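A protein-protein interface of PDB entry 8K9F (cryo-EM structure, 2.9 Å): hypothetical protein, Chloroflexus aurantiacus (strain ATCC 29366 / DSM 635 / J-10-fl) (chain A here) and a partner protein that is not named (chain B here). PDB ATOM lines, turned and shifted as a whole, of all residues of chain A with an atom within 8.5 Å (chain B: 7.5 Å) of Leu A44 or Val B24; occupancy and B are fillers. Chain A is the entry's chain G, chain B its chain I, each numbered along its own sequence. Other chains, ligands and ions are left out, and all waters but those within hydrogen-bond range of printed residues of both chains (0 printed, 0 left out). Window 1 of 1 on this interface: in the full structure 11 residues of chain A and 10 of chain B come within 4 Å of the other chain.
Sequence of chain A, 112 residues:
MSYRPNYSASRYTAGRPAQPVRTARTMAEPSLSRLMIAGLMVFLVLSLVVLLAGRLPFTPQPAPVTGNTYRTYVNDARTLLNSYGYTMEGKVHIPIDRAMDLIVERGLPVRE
The side-chain hydroxyl (OG) of Ser A47 lies within hydrogen-bond range of the backbone carbonyl oxygen (O) of Phe A43. O of Leu A44 is in hydrogen-bond range of OG of Ser A47 (2.8 Å).
Among the printed residues, pairs that only touch across the chains: Ser A47 with Leu B28, Leu A51 with Trp B31, Phe A43 with Val B24, Leu A40 with Thr B21, Ile A37 with Leu B20, Leu A40 with Leu B20, Leu A44 with Val B24, Leu A48 with Trp B31 and Leu A40 with Val B24.
Of chain B, only Val B24 (3.7 Å) comes within 4 Å of Leu A44. Val B24 touches just these residues of chain A: Leu A40, Phe A43 and Leu A44. No residue of chain A comes within 4 Å of Gly B22. Printed residues of chain B within 4 Å of Leu A51: Trp B31 (3.6 Å). Of the printed residues of chain A, Leu B20 touches Ile A37 (3.7 Å) and Leu A40 (3.7 Å). Printed residues of chain B within 4 Å of Phe A43: Val B24 (3.6 Å). Printed residues of chain B within 4 Å of Leu A40: Leu B20 (3.7 Å), Thr B21 (3.6 Å) and Val B24 (3.8 Å). Leu B27 touches none of the printed residues of chain A.
Hydrophobic or aromatic side chains of chain B that line the printed part of chain A: Leu B20, Val B24, Leu B28 and Trp B31. Of the 15 printed residues of chain A, 7 touch a printed residue of chain B. Printed residues of chain A that touch a printed residue of chain B: Ile A37, Leu A40, Phe A43, Leu A44, Ser A47, Leu A48 and Leu A51. Hydrophobic or aromatic side chains of chain A that line the printed part of chain B: Ile A37, Leu A40, Phe A43, Leu A44, Leu A48 and Leu A51.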
ATOM      1  N   ILE A  37     -17.996  15.941 -16.319  1.00  0.00           N
ATOM      2  CA  ILE A  37     -17.804  17.091 -17.207  1.00  0.00           C
ATOM      3  C   ILE A  37     -17.403  18.324 -16.411  1.00  0.00           C
ATOM      4  O   ILE A  37     -16.495  19.055 -16.808  1.00  0.00           O
ATOM      5  CB  ILE A  37     -19.067  17.390 -18.043  1.00  0.00           C
ATOM      6  CG1 ILE A  37     -19.693  16.137 -18.650  1.00  0.00           C
ATOM      7  CG2 ILE A  37     -18.732  18.373 -19.157  1.00  0.00           C
ATOM      8  CD1 ILE A  37     -18.808  15.360 -19.566  1.00  0.00           C
ATOM      9  N   ALA A  38     -18.071  18.572 -15.281  1.00  0.00           N
ATOM     10  CA  ALA A  38     -17.796  19.775 -14.501  1.00  0.00           C
ATOM     11  C   ALA A  38     -16.416  19.725 -13.858  1.00  0.00           C
ATOM     12  O   ALA A  38     -15.687  20.725 -13.873  1.00  0.00           O
ATOM     13  CB  ALA A  38     -18.877  19.973 -13.440  1.00  0.00           C
ATOM     14  N   GLY A  39     -16.031  18.567 -13.314  1.00  0.00           N
ATOM     15  CA  GLY A  39     -14.699  18.427 -12.751  1.00  0.00           C
ATOM     16  C   GLY A  39     -13.606  18.523 -13.795  1.00  0.00           C
ATOM     17  O   GLY A  39     -12.559  19.131 -13.551  1.00  0.00           O
ATOM     18  N   LEU A  40     -13.842  17.963 -14.986  1.00  0.00           N
ATOM     19  CA  LEU A  40     -12.833  18.065 -16.032  1.00  0.00           C
ATOM     20  C   LEU A  40     -12.779  19.469 -16.624  1.00  0.00           C
ATOM     21  O   LEU A  40     -11.707  19.932 -17.010  1.00  0.00           O
ATOM     22  CB  LEU A  40     -13.071  16.999 -17.101  1.00  0.00           C
ATOM     23  CG  LEU A  40     -12.042  17.013 -18.228  1.00  0.00           C
ATOM     24  CD1 LEU A  40     -11.080  15.913 -18.003  1.00  0.00           C
ATOM     25  CD2 LEU A  40     -12.719  16.857 -19.580  1.00  0.00           C
ATOM     26  N   MET A  41     -13.900  20.188 -16.654  1.00  0.00           N
ATOM     27  CA  MET A  41     -13.845  21.574 -17.103  1.00  0.00           C
ATOM     28  C   MET A  41     -13.156  22.470 -16.083  1.00  0.00           C
ATOM     29  O   MET A  41     -12.448  23.404 -16.473  1.00  0.00           O
ATOM     30  CB  MET A  41     -15.246  22.098 -17.414  1.00  0.00           C
ATOM     31  CG  MET A  41     -15.807  21.599 -18.735  1.00  0.00           C
ATOM     32  SD  MET A  41     -17.520  22.063 -19.069  1.00  0.00           S
ATOM     33  CE  MET A  41     -18.100  22.591 -17.459  1.00  0.00           C
ATOM     34  N   VAL A  42     -13.334  22.194 -14.787  1.00  0.00           N
ATOM     35  CA  VAL A  42     -12.596  22.927 -13.759  1.00  0.00           C
ATOM     36  C   VAL A  42     -11.104  22.632 -13.862  1.00  0.00           C
ATOM     37  O   VAL A  42     -10.270  23.546 -13.803  1.00  0.00           O
ATOM     38  CB  VAL A  42     -13.159  22.592 -12.364  1.00  0.00           C
ATOM     39  CG1 VAL A  42     -12.176  22.968 -11.253  1.00  0.00           C
ATOM     40  CG2 VAL A  42     -14.480  23.297 -12.156  1.00  0.00           C
ATOM     41  N   PHE A  43     -10.752  21.358 -14.058  1.00  0.00           N
ATOM     42  CA  PHE A  43      -9.361  20.967 -14.258  1.00  0.00           C
ATOM     43  C   PHE A  43      -8.786  21.569 -15.537  1.00  0.00           C
ATOM     44  O   PHE A  43      -7.625  21.976 -15.555  1.00  0.00           O
ATOM     45  CB  PHE A  43      -9.271  19.432 -14.232  1.00  0.00           C
ATOM     46  CG  PHE A  43      -8.241  18.834 -15.156  1.00  0.00           C
ATOM     47  CD1 PHE A  43      -6.945  18.620 -14.717  1.00  0.00           C
ATOM     48  CD2 PHE A  43      -8.594  18.391 -16.428  1.00  0.00           C
ATOM     49  CE1 PHE A  43      -6.001  18.047 -15.551  1.00  0.00           C
ATOM     50  CE2 PHE A  43      -7.654  17.822 -17.262  1.00  0.00           C
ATOM     51  CZ  PHE A  43      -6.360  17.646 -16.826  1.00  0.00           C
ATOM     52  N   LEU A  44      -9.594  21.659 -16.596  1.00  0.00           N
ATOM     53  CA  LEU A  44      -9.176  22.275 -17.851  1.00  0.00           C
ATOM     54  C   LEU A  44      -8.915  23.763 -17.690  1.00  0.00           C
ATOM     55  O   LEU A  44      -7.909  24.272 -18.188  1.00  0.00           O
ATOM     56  CB  LEU A  44     -10.243  22.046 -18.919  1.00  0.00           C
ATOM     57  CG  LEU A  44      -9.986  22.622 -20.314  1.00  0.00           C
ATOM     58  CD1 LEU A  44      -9.602  21.550 -21.312  1.00  0.00           C
ATOM     59  CD2 LEU A  44     -11.213  23.386 -20.793  1.00  0.00           C
ATOM     60  N   VAL A  45      -9.809  24.473 -17.000  1.00  0.00           N
ATOM     61  CA  VAL A  45      -9.635  25.909 -16.803  1.00  0.00           C
ATOM     62  C   VAL A  45      -8.437  26.184 -15.901  1.00  0.00           C
ATOM     63  O   VAL A  45      -7.613  27.058 -16.196  1.00  0.00           O
ATOM     64  CB  VAL A  45     -10.936  26.529 -16.259  1.00  0.00           C
ATOM     65  CG1 VAL A  45     -10.698  27.926 -15.712  1.00  0.00           C
ATOM     66  CG2 VAL A  45     -11.991  26.580 -17.357  1.00  0.00           C
ATOM     67  N   LEU A  46      -8.289  25.409 -14.822  1.00  0.00           N
ATOM     68  CA  LEU A  46      -7.180  25.619 -13.897  1.00  0.00           C
ATOM     69  C   LEU A  46      -5.850  25.241 -14.542  1.00  0.00           C
ATOM     70  O   LEU A  46      -4.847  25.943 -14.369  1.00  0.00           O
ATOM     71  CB  LEU A  46      -7.391  24.813 -12.613  1.00  0.00           C
ATOM     72  CG  LEU A  46      -6.267  24.883 -11.577  1.00  0.00           C
ATOM     73  CD1 LEU A  46      -6.096  26.305 -11.065  1.00  0.00           C
ATOM     74  CD2 LEU A  46      -6.531  23.922 -10.428  1.00  0.00           C
ATOM     75  N   SER A  47      -5.840  24.171 -15.337  1.00  0.00           N
ATOM     76  CA  SER A  47      -4.648  23.760 -16.062  1.00  0.00           C
ATOM     77  C   SER A  47      -4.280  24.737 -17.167  1.00  0.00           C
ATOM     78  O   SER A  47      -3.095  24.961 -17.420  1.00  0.00           O
ATOM     79  CB  SER A  47      -4.875  22.378 -16.658  1.00  0.00           C
ATOM     80  OG  SER A  47      -5.821  22.448 -17.703  1.00  0.00           O
ATOM     81  N   LEU A  48      -5.272  25.306 -17.852  1.00  0.00           N
ATOM     82  CA  LEU A  48      -4.990  26.268 -18.907  1.00  0.00           C
ATOM     83  C   LEU A  48      -4.510  27.588 -18.321  1.00  0.00           C
ATOM     84  O   LEU A  48      -3.654  28.258 -18.906  1.00  0.00           O
ATOM     85  CB  LEU A  48      -6.238  26.464 -19.766  1.00  0.00           C
ATOM     86  CG  LEU A  48      -6.233  25.743 -21.111  1.00  0.00           C
ATOM     87  CD1 LEU A  48      -7.510  26.029 -21.881  1.00  0.00           C
ATOM     88  CD2 LEU A  48      -5.011  26.139 -21.926  1.00  0.00           C
ATOM     89  N   VAL A  49      -5.033  27.956 -17.146  1.00  0.00           N
ATOM     90  CA  VAL A  49      -4.520  29.106 -16.405  1.00  0.00           C
ATOM     91  C   VAL A  49      -3.084  28.849 -15.961  1.00  0.00           C
ATOM     92  O   VAL A  49      -2.234  29.744 -16.015  1.00  0.00           O
ATOM     93  CB  VAL A  49      -5.462  29.421 -15.221  1.00  0.00           C
ATOM     94  CG1 VAL A  49      -4.766  30.189 -14.103  1.00  0.00           C
ATOM     95  CG2 VAL A  49      -6.667  30.205 -15.710  1.00  0.00           C
ATOM     96  N   VAL A  50      -2.777  27.608 -15.576  1.00  0.00           N
ATOM     97  CA  VAL A  50      -1.408  27.232 -15.225  1.00  0.00           C
ATOM     98  C   VAL A  50      -0.476  27.282 -16.436  1.00  0.00           C
ATOM     99  O   VAL A  50       0.659  27.770 -16.331  1.00  0.00           O
ATOM    100  CB  VAL A  50      -1.440  25.847 -14.554  1.00  0.00           C
ATOM    101  CG1 VAL A  50      -0.145  25.069 -14.764  1.00  0.00           C
ATOM    102  CG2 VAL A  50      -1.736  26.021 -13.086  1.00  0.00           C
ATOM    103  N   LEU A  51      -0.941  26.798 -17.593  1.00  0.00           N
ATOM    104  CA  LEU A  51      -0.168  26.875 -18.831  1.00  0.00           C
ATOM    105  C   LEU A  51       0.101  28.321 -19.225  1.00  0.00           C
ATOM    106  O   LEU A  51       1.205  28.656 -19.662  1.00  0.00           O
ATOM    107  CB  LEU A  51      -0.911  26.163 -19.962  1.00  0.00           C
ATOM    108  CG  LEU A  51      -0.435  24.822 -20.522  1.00  0.00           C
ATOM    109  CD1 LEU A  51      -0.727  23.689 -19.570  1.00  0.00           C
ATOM    110  CD2 LEU A  51      -1.085  24.568 -21.871  1.00  0.00           C
ATOM    111  N   VAL B  18     -14.913   9.248 -20.032  1.00  0.00           N
ATOM    112  CA  VAL B  18     -13.549   8.708 -19.928  1.00  0.00           C
ATOM    113  C   VAL B  18     -12.722   9.073 -21.158  1.00  0.00           C
ATOM    114  O   VAL B  18     -11.553   9.456 -21.043  1.00  0.00           O
ATOM    115  CB  VAL B  18     -13.524   7.186 -19.690  1.00  0.00           C
ATOM    116  CG1 VAL B  18     -12.189   6.798 -19.084  1.00  0.00           C
ATOM    117  CG2 VAL B  18     -14.587   6.762 -18.733  1.00  0.00           C
ATOM    118  N   THR B  19     -13.308   8.989 -22.350  1.00  0.00           N
ATOM    119  CA  THR B  19     -12.551   9.418 -23.515  1.00  0.00           C
ATOM    120  C   THR B  19     -12.450  10.939 -23.622  1.00  0.00           C
ATOM    121  O   THR B  19     -11.441  11.429 -24.129  1.00  0.00           O
ATOM    122  CB  THR B  19     -13.120   8.786 -24.801  1.00  0.00           C
ATOM    123  OG1 THR B  19     -12.099   8.748 -25.807  1.00  0.00           O
ATOM    124  CG2 THR B  19     -14.337   9.519 -25.351  1.00  0.00           C
ATOM    125  N   LEU B  20     -13.417  11.707 -23.102  1.00  0.00           N
ATOM    126  CA  LEU B  20     -13.245  13.155 -23.112  1.00  0.00           C
ATOM    127  C   LEU B  20     -12.232  13.602 -22.064  1.00  0.00           C
ATOM    128  O   LEU B  20     -11.553  14.611 -22.267  1.00  0.00           O
ATOM    129  CB  LEU B  20     -14.603  13.847 -22.926  1.00  0.00           C
ATOM    130  CG  LEU B  20     -14.845  15.233 -22.315  1.00  0.00           C
ATOM    131  CD1 LEU B  20     -14.171  16.365 -23.084  1.00  0.00           C
ATOM    132  CD2 LEU B  20     -16.331  15.472 -22.283  1.00  0.00           C
ATOM    133  N   THR B  21     -12.090  12.847 -20.976  1.00  0.00           N
ATOM    134  CA  THR B  21     -10.953  12.931 -20.075  1.00  0.00           C
ATOM    135  C   THR B  21      -9.633  12.613 -20.742  1.00  0.00           C
ATOM    136  O   THR B  21      -8.664  13.339 -20.511  1.00  0.00           O
ATOM    137  CB  THR B  21     -11.127  11.975 -18.892  1.00  0.00           C
ATOM    138  OG1 THR B  21     -12.503  11.909 -18.501  1.00  0.00           O
ATOM    139  CG2 THR B  21     -10.233  12.365 -17.730  1.00  0.00           C
ATOM    140  N   GLY B  22      -9.572  11.533 -21.519  1.00  0.00           N
ATOM    141  CA  GLY B  22      -8.354  11.139 -22.193  1.00  0.00           C
ATOM    142  C   GLY B  22      -7.888  12.161 -23.208  1.00  0.00           C
ATOM    143  O   GLY B  22      -6.730  12.582 -23.173  1.00  0.00           O
ATOM    144  N   MET B  23      -8.799  12.629 -24.064  1.00  0.00           N
ATOM    145  CA  MET B  23      -8.423  13.610 -25.074  1.00  0.00           C
ATOM    146  C   MET B  23      -8.242  15.010 -24.507  1.00  0.00           C
ATOM    147  O   MET B  23      -7.812  15.901 -25.240  1.00  0.00           O
ATOM    148  CB  MET B  23      -9.437  13.656 -26.224  1.00  0.00           C
ATOM    149  CG  MET B  23      -9.868  12.308 -26.766  1.00  0.00           C
ATOM    150  SD  MET B  23      -8.681  10.983 -26.470  1.00  0.00           S
ATOM    151  CE  MET B  23      -7.620  11.145 -27.903  1.00  0.00           C
ATOM    152  N   VAL B  24      -8.569  15.241 -23.239  1.00  0.00           N
ATOM    153  CA  VAL B  24      -8.206  16.515 -22.632  1.00  0.00           C
ATOM    154  C   VAL B  24      -6.867  16.398 -21.915  1.00  0.00           C
ATOM    155  O   VAL B  24      -5.936  17.162 -22.189  1.00  0.00           O
ATOM    156  CB  VAL B  24      -9.328  17.012 -21.699  1.00  0.00           C
ATOM    157  CG1 VAL B  24      -8.798  17.979 -20.664  1.00  0.00           C
ATOM    158  CG2 VAL B  24     -10.407  17.689 -22.514  1.00  0.00           C
ATOM    159  N   ALA B  25      -6.731  15.405 -21.031  1.00  0.00           N
ATOM    160  CA  ALA B  25      -5.533  15.277 -20.211  1.00  0.00           C
ATOM    161  C   ALA B  25      -4.316  14.860 -21.026  1.00  0.00           C
ATOM    162  O   ALA B  25      -3.253  15.480 -20.901  1.00  0.00           O
ATOM    163  CB  ALA B  25      -5.779  14.278 -19.083  1.00  0.00           C
ATOM    164  N   PHE B  26      -4.449  13.822 -21.865  1.00  0.00           N
ATOM    165  CA  PHE B  26      -3.320  13.355 -22.661  1.00  0.00           C
ATOM    166  C   PHE B  26      -2.894  14.397 -23.688  1.00  0.00           C
ATOM    167  O   PHE B  26      -1.696  14.582 -23.926  1.00  0.00           O
ATOM    168  CB  PHE B  26      -3.674  12.032 -23.350  1.00  0.00           C
ATOM    169  CG  PHE B  26      -2.854  11.748 -24.576  1.00  0.00           C
ATOM    170  CD1 PHE B  26      -1.532  11.345 -24.459  1.00  0.00           C
ATOM    171  CD2 PHE B  26      -3.402  11.886 -25.847  1.00  0.00           C
ATOM    172  CE1 PHE B  26      -0.768  11.089 -25.580  1.00  0.00           C
ATOM    173  CE2 PHE B  26      -2.642  11.639 -26.972  1.00  0.00           C
ATOM    174  CZ  PHE B  26      -1.324  11.236 -26.837  1.00  0.00           C
ATOM    175  N   LEU B  27      -3.856  15.095 -24.299  1.00  0.00           N
ATOM    176  CA  LEU B  27      -3.488  16.158 -25.227  1.00  0.00           C
ATOM    177  C   LEU B  27      -2.900  17.357 -24.498  1.00  0.00           C
ATOM    178  O   LEU B  27      -2.112  18.102 -25.085  1.00  0.00           O
ATOM    179  CB  LEU B  27      -4.684  16.586 -26.076  1.00  0.00           C
ATOM    180  CG  LEU B  27      -5.078  15.633 -27.210  1.00  0.00           C
ATOM    181  CD1 LEU B  27      -6.198  16.224 -28.062  1.00  0.00           C
ATOM    182  CD2 LEU B  27      -3.876  15.253 -28.071  1.00  0.00           C
ATOM    183  N   LEU B  28      -3.243  17.551 -23.224  1.00  0.00           N
ATOM    184  CA  LEU B  28      -2.589  18.594 -22.445  1.00  0.00           C
ATOM    185  C   LEU B  28      -1.132  18.248 -22.162  1.00  0.00           C
ATOM    186  O   LEU B  28      -0.260  19.122 -22.231  1.00  0.00           O
ATOM    187  CB  LEU B  28      -3.367  18.828 -21.154  1.00  0.00           C
ATOM    188  CG  LEU B  28      -4.361  19.984 -21.253  1.00  0.00           C
ATOM    189  CD1 LEU B  28      -5.019  20.206 -19.925  1.00  0.00           C
ATOM    190  CD2 LEU B  28      -3.672  21.256 -21.706  1.00  0.00           C
ATOM    191  N   MET B  29      -0.847  16.975 -21.854  1.00  0.00           N
ATOM    192  CA  MET B  29       0.553  16.550 -21.752  1.00  0.00           C
ATOM    193  C   MET B  29       1.261  16.616 -23.100  1.00  0.00           C
ATOM    194  O   MET B  29       2.472  16.848 -23.152  1.00  0.00           O
ATOM    195  CB  MET B  29       0.689  15.137 -21.178  1.00  0.00           C
ATOM    196  CG  MET B  29      -0.271  14.751 -20.097  1.00  0.00           C
ATOM    197  SD  MET B  29       0.519  13.774 -18.816  1.00  0.00           S
ATOM    198  CE  MET B  29      -0.861  13.498 -17.720  1.00  0.00           C
ATOM    199  N   VAL B  30       0.530  16.407 -24.194  1.00  0.00           N
ATOM    200  CA  VAL B  30       1.124  16.544 -25.521  1.00  0.00           C
ATOM    201  C   VAL B  30       1.483  18.001 -25.799  1.00  0.00           C
ATOM    202  O   VAL B  30       2.570  18.299 -26.314  1.00  0.00           O
ATOM    203  CB  VAL B  30       0.174  15.959 -26.585  1.00  0.00           C
ATOM    204  CG1 VAL B  30       0.384  16.592 -27.955  1.00  0.00           C
ATOM    205  CG2 VAL B  30       0.362  14.470 -26.672  1.00  0.00           C
ATOM    206  N   TRP B  31       0.592  18.929 -25.436  1.00  0.00           N
ATOM    207  CA  TRP B  31       0.838  20.350 -25.664  1.00  0.00           C
ATOM    208  C   TRP B  31       1.989  20.834 -24.790  1.00  0.00           C
ATOM    209  O   TRP B  31       2.870  21.552 -25.272  1.00  0.00           O
ATOM    210  CB  TRP B  31      -0.466  21.132 -25.411  1.00  0.00           C
ATOM    211  CG  TRP B  31      -0.502  22.688 -25.438  1.00  0.00           C
ATOM    212  CD1 TRP B  31       0.543  23.573 -25.506  1.00  0.00           C
ATOM    213  CD2 TRP B  31      -1.691  23.497 -25.396  1.00  0.00           C
ATOM    214  NE1 TRP B  31       0.081  24.865 -25.505  1.00  0.00           N
ATOM    215  CE2 TRP B  31      -1.286  24.846 -25.442  1.00  0.00           C
ATOM    216  CE3 TRP B  31      -3.058  23.206 -25.328  1.00  0.00           C
ATOM    217  CZ2 TRP B  31      -2.199  25.899 -25.419  1.00  0.00           C
ATOM    218  CZ3 TRP B  31      -3.959  24.252 -25.306  1.00  0.00           C
ATOM    219  CH2 TRP B  31      -3.527  25.583 -25.349  1.00  0.00           C
